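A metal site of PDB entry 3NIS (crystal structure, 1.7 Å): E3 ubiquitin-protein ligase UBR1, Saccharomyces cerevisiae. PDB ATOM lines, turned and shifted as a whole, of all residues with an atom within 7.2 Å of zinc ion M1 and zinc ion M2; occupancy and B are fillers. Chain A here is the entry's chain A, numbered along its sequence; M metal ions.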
ATOM      1  N   HIS A   4      13.802  23.413  21.404  1.00  0.00           N
ATOM      2  CA  HIS A   4      13.320  23.842  20.106  1.00  0.00           C
ATOM      3  C   HIS A   4      11.925  23.266  19.956  1.00  0.00           C
ATOM      4  O   HIS A   4      11.754  22.054  19.800  1.00  0.00           O
ATOM      5  CB  HIS A   4      14.240  23.371  18.979  1.00  0.00           C
ATOM      6  CG  HIS A   4      14.157  24.217  17.740  1.00  0.00           C
ATOM      7  ND1 HIS A   4      13.010  24.318  16.982  1.00  0.00           N
ATOM      8  CD2 HIS A   4      15.088  24.974  17.120  1.00  0.00           C
ATOM      9  CE1 HIS A   4      13.245  25.116  15.951  1.00  0.00           C
ATOM     10  NE2 HIS A   4      14.495  25.526  16.010  1.00  0.00           N
ATOM     11  N   LYS A   5      10.937  24.140  20.053  1.00  0.00           N
ATOM     12  CA  LYS A   5       9.547  23.725  20.034  1.00  0.00           C
ATOM     13  C   LYS A   5       9.105  23.472  18.617  1.00  0.00           C
ATOM     14  O   LYS A   5       9.644  24.077  17.665  1.00  0.00           O
ATOM     15  CB  LYS A   5       8.673  24.808  20.669  1.00  0.00           C
ATOM     16  CG  LYS A   5       9.127  25.208  22.058  1.00  0.00           C
ATOM     17  CD  LYS A   5       8.335  26.386  22.556  1.00  0.00           C
ATOM     18  CE  LYS A   5       8.845  26.832  23.907  1.00  0.00           C
ATOM     19  NZ  LYS A   5       7.966  27.901  24.462  1.00  0.00           N
ATOM     20  N   HIS A   6       8.125  22.587  18.465  1.00  0.00           N
ATOM     21  CA  HIS A   6       7.507  22.339  17.168  1.00  0.00           C
ATOM     22  C   HIS A   6       6.027  22.737  17.201  1.00  0.00           C
ATOM     23  O   HIS A   6       5.177  22.070  16.621  1.00  0.00           O
ATOM     24  CB  HIS A   6       7.670  20.879  16.766  1.00  0.00           C
ATOM     25  CG  HIS A   6       7.077  19.916  17.737  1.00  0.00           C
ATOM     26  ND1 HIS A   6       5.740  19.555  17.692  1.00  0.00           N
ATOM     27  CD2 HIS A   6       7.616  19.240  18.778  1.00  0.00           C
ATOM     28  CE1 HIS A   6       5.493  18.699  18.674  1.00  0.00           C
ATOM     29  NE2 HIS A   6       6.613  18.492  19.344  1.00  0.00           N
ATOM     30  N   ARG A   9       2.638  21.973  14.846  1.00  0.00           N
ATOM     31  CA  ARG A   9       2.927  20.845  13.973  1.00  0.00           C
ATOM     32  C   ARG A   9       3.443  19.652  14.761  1.00  0.00           C
ATOM     33  O   ARG A   9       3.591  19.719  15.996  1.00  0.00           O
ATOM     34  CB  ARG A   9       3.911  21.224  12.855  1.00  0.00           C
ATOM     35  CG  ARG A   9       5.199  21.889  13.340  1.00  0.00           C
ATOM     36  CD  ARG A   9       6.305  21.714  12.341  1.00  0.00           C
ATOM     37  NE  ARG A   9       6.892  20.368  12.393  1.00  0.00           N
ATOM     38  CZ  ARG A   9       7.992  20.015  11.744  1.00  0.00           C
ATOM     39  NH1 ARG A   9       8.623  20.890  10.956  1.00  0.00           N
ATOM     40  NH2 ARG A   9       8.472  18.789  11.865  1.00  0.00           N
ATOM     41  N   ASN A  10       3.685  18.552  14.060  1.00  0.00           N
ATOM     42  CA  ASN A  10       4.261  17.356  14.655  1.00  0.00           C
ATOM     43  C   ASN A  10       5.760  17.548  14.904  1.00  0.00           C
ATOM     44  O   ASN A  10       6.389  18.431  14.312  1.00  0.00           O
ATOM     45  CB  ASN A  10       4.078  16.169  13.712  1.00  0.00           C
ATOM     46  CG  ASN A  10       4.892  16.326  12.437  1.00  0.00           C
ATOM     47  OD1 ASN A  10       4.768  17.327  11.738  1.00  0.00           O
ATOM     48  ND2 ASN A  10       5.746  15.346  12.143  1.00  0.00           N
ATOM     49  N   CYS A  11       6.328  16.697  15.749  1.00  0.00           N
ATOM     50  CA  CYS A  11       7.777  16.691  15.961  1.00  0.00           C
ATOM     51  C   CYS A  11       8.502  16.094  14.740  1.00  0.00           C
ATOM     52  O   CYS A  11       9.189  16.817  13.999  1.00  0.00           O
ATOM     53  CB  CYS A  11       8.137  15.941  17.240  1.00  0.00           C
ATOM     54  SG  CYS A  11       9.917  15.793  17.491  1.00  0.00           S
ATOM     55  N   GLY A  12       8.312  14.794  14.532  1.00  0.00           N
ATOM     56  CA  GLY A  12       8.888  14.093  13.373  1.00  0.00           C
ATOM     57  C   GLY A  12      10.404  13.975  13.392  1.00  0.00           C
ATOM     58  O   GLY A  12      11.013  13.615  12.377  1.00  0.00           O
ATOM     59  N   ARG A  13      11.013  14.276  14.531  1.00  0.00           N
ATOM     60  CA  ARG A  13      12.468  14.169  14.692  1.00  0.00           C
ATOM     61  C   ARG A  13      12.937  12.719  14.550  1.00  0.00           C
ATOM     62  O   ARG A  13      12.401  11.819  15.191  1.00  0.00           O
ATOM     63  CB  ARG A  13      12.870  14.717  16.069  1.00  0.00           C
ATOM     64  CG  ARG A  13      14.354  14.695  16.402  1.00  0.00           C
ATOM     65  CD  ARG A  13      14.555  15.254  17.822  1.00  0.00           C
ATOM     66  NE  ARG A  13      15.928  15.179  18.314  1.00  0.00           N
ATOM     67  CZ  ARG A  13      16.471  14.106  18.909  1.00  0.00           C
ATOM     68  NH1 ARG A  13      15.754  12.993  19.074  1.00  0.00           N
ATOM     69  NH2 ARG A  13      17.732  14.150  19.327  1.00  0.00           N
ATOM     70  N   PHE A  15      15.319   9.730  15.379  1.00  0.00           N
ATOM     71  CA  PHE A  15      16.056   9.376  16.587  1.00  0.00           C
ATOM     72  C   PHE A  15      17.549   9.275  16.315  1.00  0.00           C
ATOM     73  O   PHE A  15      17.974   8.891  15.231  1.00  0.00           O
ATOM     74  CB  PHE A  15      15.531   8.071  17.163  1.00  0.00           C
ATOM     75  CG  PHE A  15      14.157   8.191  17.724  1.00  0.00           C
ATOM     76  CD1 PHE A  15      13.950   8.673  19.011  1.00  0.00           C
ATOM     77  CD2 PHE A  15      13.051   7.838  16.959  1.00  0.00           C
ATOM     78  CE1 PHE A  15      12.674   8.796  19.531  1.00  0.00           C
ATOM     79  CE2 PHE A  15      11.758   7.960  17.475  1.00  0.00           C
ATOM     80  CZ  PHE A  15      11.577   8.429  18.763  1.00  0.00           C
ATOM     81  N   VAL A  34       5.678   6.479  19.164  1.00  0.00           N
ATOM     82  CA  VAL A  34       6.849   6.761  20.001  1.00  0.00           C
ATOM     83  C   VAL A  34       7.098   8.255  20.180  1.00  0.00           C
ATOM     84  O   VAL A  34       6.643   9.081  19.378  1.00  0.00           O
ATOM     85  CB  VAL A  34       8.123   6.067  19.463  1.00  0.00           C
ATOM     86  CG1 VAL A  34       8.009   4.545  19.584  1.00  0.00           C
ATOM     87  CG2 VAL A  34       8.412   6.507  18.006  1.00  0.00           C
ATOM     88  N   LEU A  35       7.824   8.578  21.235  1.00  0.00           N
ATOM     89  CA  LEU A  35       8.139   9.962  21.587  1.00  0.00           C
ATOM     90  C   LEU A  35       9.626  10.083  21.850  1.00  0.00           C
ATOM     91  O   LEU A  35      10.231   9.162  22.397  1.00  0.00           O
ATOM     92  CB  LEU A  35       7.381  10.370  22.851  1.00  0.00           C
ATOM     93  CG  LEU A  35       5.865  10.500  22.739  1.00  0.00           C
ATOM     94  CD1 LEU A  35       5.233  10.585  24.132  1.00  0.00           C
ATOM     95  CD2 LEU A  35       5.477  11.691  21.884  1.00  0.00           C
ATOM     96  N   CYS A  36      10.201  11.217  21.472  1.00  0.00           N
ATOM     97  CA  CYS A  36      11.619  11.478  21.645  1.00  0.00           C
ATOM     98  C   CYS A  36      11.892  12.161  22.987  1.00  0.00           C
ATOM     99  O   CYS A  36      10.955  12.591  23.687  1.00  0.00           O
ATOM    100  CB  CYS A  36      12.154  12.347  20.501  1.00  0.00           C
ATOM    101  SG  CYS A  36      11.812  14.113  20.669  1.00  0.00           S
ATOM    102  N   ILE A  37      13.168  12.291  23.313  1.00  0.00           N
ATOM    103  CA  ILE A  37      13.591  12.875  24.600  1.00  0.00           C
ATOM    104  C   ILE A  37      13.202  14.345  24.770  1.00  0.00           C
ATOM    105  O   ILE A  37      13.053  14.838  25.891  1.00  0.00           O
ATOM    106  CB  ILE A  37      15.106  12.720  24.839  1.00  0.00           C
ATOM    107  CG1 ILE A  37      15.888  13.209  23.604  1.00  0.00           C
ATOM    108  CG2 ILE A  37      15.449  11.283  25.165  1.00  0.00           C
ATOM    109  CD1 ILE A  37      17.227  13.840  23.895  1.00  0.00           C
ATOM    110  N   HIS A  38      13.059  15.048  23.643  1.00  0.00           N
ATOM    111  CA  HIS A  38      12.676  16.456  23.631  1.00  0.00           C
ATOM    112  C   HIS A  38      11.200  16.629  24.002  1.00  0.00           C
ATOM    113  O   HIS A  38      10.802  17.677  24.517  1.00  0.00           O
ATOM    114  CB  HIS A  38      12.875  17.067  22.239  1.00  0.00           C
ATOM    115  CG  HIS A  38      14.291  17.114  21.772  1.00  0.00           C
ATOM    116  ND1 HIS A  38      15.325  16.485  22.421  1.00  0.00           N
ATOM    117  CD2 HIS A  38      14.847  17.715  20.687  1.00  0.00           C
ATOM    118  CE1 HIS A  38      16.454  16.707  21.775  1.00  0.00           C
ATOM    119  NE2 HIS A  38      16.194  17.450  20.722  1.00  0.00           N
ATOM    120  N   CYS A  39      10.405  15.588  23.770  1.00  0.00           N
ATOM    121  CA  CYS A  39       8.950  15.689  23.780  1.00  0.00           C
ATOM    122  C   CYS A  39       8.282  14.934  24.919  1.00  0.00           C
ATOM    123  O   CYS A  39       7.266  15.386  25.477  1.00  0.00           O
ATOM    124  CB  CYS A  39       8.402  15.155  22.463  1.00  0.00           C
ATOM    125  SG  CYS A  39       8.793  16.208  21.056  1.00  0.00           S
ATOM    126  N   PHE A  40       8.824  13.766  25.240  1.00  0.00           N
ATOM    127  CA  PHE A  40       8.251  12.941  26.285  1.00  0.00           C
ATOM    128  C   PHE A  40       8.139  13.707  27.598  1.00  0.00           C
ATOM    129  O   PHE A  40       9.142  14.188  28.128  1.00  0.00           O
ATOM    130  CB  PHE A  40       9.069  11.653  26.470  1.00  0.00           C
ATOM    131  CG  PHE A  40       8.527  10.765  27.547  1.00  0.00           C
ATOM    132  CD1 PHE A  40       7.483   9.874  27.278  1.00  0.00           C
ATOM    133  CD2 PHE A  40       9.041  10.825  28.853  1.00  0.00           C
ATOM    134  CE1 PHE A  40       6.988   9.059  28.258  1.00  0.00           C
ATOM    135  CE2 PHE A  40       8.541  10.002  29.860  1.00  0.00           C
ATOM    136  CZ  PHE A  40       7.502   9.119  29.564  1.00  0.00           C
ATOM    137  N   ILE A  62      10.823   8.038  13.734  1.00  0.00           N
ATOM    138  CA  ILE A  62      10.588   9.455  13.968  1.00  0.00           C
ATOM    139  C   ILE A  62       9.593   9.670  15.118  1.00  0.00           C
ATOM    140  O   ILE A  62       8.691   8.853  15.337  1.00  0.00           O
ATOM    141  CB  ILE A  62      10.115  10.185  12.671  1.00  0.00           C
ATOM    142  CG1 ILE A  62       8.797   9.614  12.133  1.00  0.00           C
ATOM    143  CG2 ILE A  62      11.199  10.153  11.605  1.00  0.00           C
ATOM    144  CD1 ILE A  62       7.548  10.428  12.539  1.00  0.00           C
ATOM    145  N   CYS A  63       9.764  10.774  15.833  1.00  0.00           N
ATOM    146  CA  CYS A  63       8.892  11.106  16.950  1.00  0.00           C
ATOM    147  C   CYS A  63       7.488  11.499  16.502  1.00  0.00           C
ATOM    148  O   CYS A  63       7.315  12.281  15.572  1.00  0.00           O
ATOM    149  CB  CYS A  63       9.524  12.248  17.744  1.00  0.00           C
ATOM    150  SG  CYS A  63       8.514  12.807  19.090  1.00  0.00           S
ATOM    151  N   ASP A  64       6.473  10.940  17.173  1.00  0.00           N
ATOM    152  CA  ASP A  64       5.088  11.173  16.808  1.00  0.00           C
ATOM    153  C   ASP A  64       4.388  12.253  17.630  1.00  0.00           C
ATOM    154  O   ASP A  64       3.170  12.438  17.513  1.00  0.00           O
ATOM    155  CB  ASP A  64       4.265   9.876  16.914  1.00  0.00           C
ATOM    156  CG  ASP A  64       4.752   8.795  16.002  1.00  0.00           C
ATOM    157  OD1 ASP A  64       4.935   9.055  14.780  1.00  0.00           O
ATOM    158  OD2 ASP A  64       4.961   7.683  16.511  1.00  0.00           O
ATOM    159  N   CYS A  65       5.148  12.960  18.468  1.00  0.00           N
ATOM    160  CA  CYS A  65       4.568  14.040  19.259  1.00  0.00           C
ATOM    161  C   CYS A  65       3.895  15.072  18.352  1.00  0.00           C
ATOM    162  O   CYS A  65       4.491  15.538  17.384  1.00  0.00           O
ATOM    163  CB  CYS A  65       5.647  14.705  20.104  1.00  0.00           C
ATOM    164  SG  CYS A  65       5.027  15.976  21.214  1.00  0.00           S
ATOM    165  N   GLY A  66       2.647  15.409  18.647  1.00  0.00           N
ATOM    166  CA  GLY A  66       1.906  16.359  17.830  1.00  0.00           C
ATOM    167  C   GLY A  66       1.225  15.755  16.619  1.00  0.00           C
ATOM    168  O   GLY A  66       0.577  16.484  15.858  1.00  0.00           O
ATOM    169  N   LEU A  75      -1.337  15.125  24.488  1.00  0.00           N
ATOM    170  CA  LEU A  75       0.024  15.183  25.016  1.00  0.00           C
ATOM    171  C   LEU A  75       0.408  16.624  25.316  1.00  0.00           C
ATOM    172  O   LEU A  75      -0.032  17.549  24.635  1.00  0.00           O
ATOM    173  CB  LEU A  75       1.043  14.556  24.048  1.00  0.00           C
ATOM    174  CG  LEU A  75       0.942  13.077  23.669  1.00  0.00           C
ATOM    175  CD1 LEU A  75       2.167  12.650  22.901  1.00  0.00           C
ATOM    176  CD2 LEU A  75       0.763  12.179  24.890  1.00  0.00           C
ATOM    177  N   HIS A  76       1.235  16.800  26.345  1.00  0.00           N
ATOM    178  CA  HIS A  76       1.759  18.126  26.673  1.00  0.00           C
ATOM    179  C   HIS A  76       3.264  18.096  26.446  1.00  0.00           C
ATOM    180  O   HIS A  76       4.043  17.743  27.318  1.00  0.00           O
ATOM    181  CB  HIS A  76       1.377  18.505  28.115  1.00  0.00           C
ATOM    182  CG  HIS A  76      -0.103  18.459  28.354  1.00  0.00           C
ATOM    183  ND1 HIS A  76      -0.741  17.312  28.784  1.00  0.00           N
ATOM    184  CD2 HIS A  76      -1.061  19.392  28.167  1.00  0.00           C
ATOM    185  CE1 HIS A  76      -2.038  17.558  28.887  1.00  0.00           C
ATOM    186  NE2 HIS A  76      -2.260  18.810  28.522  1.00  0.00           N
ATOM    187  N   CYS A  77       3.641  18.426  25.220  1.00  0.00           N
ATOM    188  CA  CYS A  77       5.015  18.344  24.774  1.00  0.00           C
ATOM    189  C   CYS A  77       5.931  18.996  25.803  1.00  0.00           C
ATOM    190  O   CYS A  77       5.711  20.137  26.183  1.00  0.00           O
ATOM    191  CB  CYS A  77       5.191  19.023  23.421  1.00  0.00           C
ATOM    192  SG  CYS A  77       6.880  18.960  22.828  1.00  0.00           S
ATOM    193  N   LYS A  78       6.948  18.257  26.238  1.00  0.00           N
ATOM    194  CA  LYS A  78       7.887  18.779  27.239  1.00  0.00           C
ATOM    195  C   LYS A  78       8.558  20.083  26.786  1.00  0.00           C
ATOM    196  O   LYS A  78       8.783  20.986  27.587  1.00  0.00           O
ATOM    197  CB  LYS A  78       8.939  17.713  27.591  1.00  0.00           C
ATOM    198  CG  LYS A  78       9.805  18.072  28.801  1.00  0.00           C
ATOM    199  CD  LYS A  78      10.533  16.844  29.317  1.00  0.00           C
ATOM    200  CE  LYS A  78      11.242  17.133  30.635  1.00  0.00           C
ATOM    201  NZ  LYS A  78      12.494  17.890  30.401  1.00  0.00           N
ATOM    202  N   ALA A  79       8.848  20.190  25.486  1.00  0.00           N
ATOM    203  CA  ALA A  79       9.485  21.389  24.921  1.00  0.00           C
ATOM    204  C   ALA A  79       8.669  22.661  25.174  1.00  0.00           C
ATOM    205  O   ALA A  79       9.232  23.738  25.300  1.00  0.00           O
ATOM    206  CB  ALA A  79       9.764  21.196  23.433  1.00  0.00           C
ATOM    207  N   GLU A  80       7.350  22.530  25.244  1.00  0.00           N
ATOM    208  CA  GLU A  80       6.459  23.681  25.417  1.00  0.00           C
ATOM    209  C   GLU A  80       6.531  24.313  26.813  1.00  0.00           C
ATOM    210  O   GLU A  80       6.120  25.457  27.003  1.00  0.00           O
ATOM    211  CB  GLU A  80       5.019  23.303  25.056  1.00  0.00           C
ATOM    212  CG  GLU A  80       4.815  22.968  23.575  1.00  0.00           C
ATOM    213  CD  GLU A  80       4.970  24.164  22.654  1.00  0.00           C
ATOM    214  OE1 GLU A  80       4.632  25.292  23.069  1.00  0.00           O
ATOM    215  OE2 GLU A  80       5.425  23.979  21.506  1.00  0.00           O
HETATM  216 ZN    ZN M   1       9.802  14.678  19.505  1.00  0.00          ZN
HETATM  217 ZN    ZN M   2       6.772  17.437  21.125  1.00  0.00          ZN
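A ring nitrogen (ND1) of His 6 is in hydrogen-bond range of the backbone carbonyl oxygen (O) of Arg 9 (2.7 Å). The backbone carbonyl oxygen (O) of Cys 65 is in hydrogen-bond range of the backbone NH (N) of Cys 11, at 2.7 Å. The side-chain sulfur (SG) of Cys 63 sits close to the backbone NH (N) of Cys 65 (3.4 Å). The backbone NH of Ala 79 sits close to the side-chain sulfur of Cys 77, 3.5 Å away. O of Cys 11 lies within hydrogen-bond range of NH2 of Arg 9, at 3.0 Å. The backbone carbonyl oxygen of Arg 13 sits at hydrogen-bond distance from the backbone NH of Cys 63. The backbone NH (N) of Gly 12 is in hydrogen-bond range of the backbone carbonyl oxygen (O) of Cys 63 (2.9 Å). The backbone carbonyl oxygen (O) of Cys 39 sits at hydrogen-bond distance from the backbone NH (N) of Lys 78 (3.0 Å).
Four residues have an atom within 4 Å of zinc ion M1: Cys 11, Cys 36, Cys 39 and Cys 63.
Of the 27 residues printed, 4 come within 4 Å of zinc ion M2. The nearest printed residue that does not touch zinc ion M2 is Cys 11 (4.4 Å).
Zinc ion M1 is bound by the side-chain sulfur of Cys 11 (2.3 Å), the side-chain sulfur of Cys 63 (2.3 Å), the side-chain sulfur of Cys 36 (2.4 Å) and the side-chain sulfur of Cys 39 (2.4 Å).
Zinc ion M2 is bound by a ring nitrogen (NE2) of His 6 (2.1 Å), the side-chain sulfur (SG) of Cys 65 (2.3 Å), the side-chain sulfur (SG) of Cys 77 (2.3 Å) and the side-chain sulfur (SG) of Cys 39 (2.4 Å).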
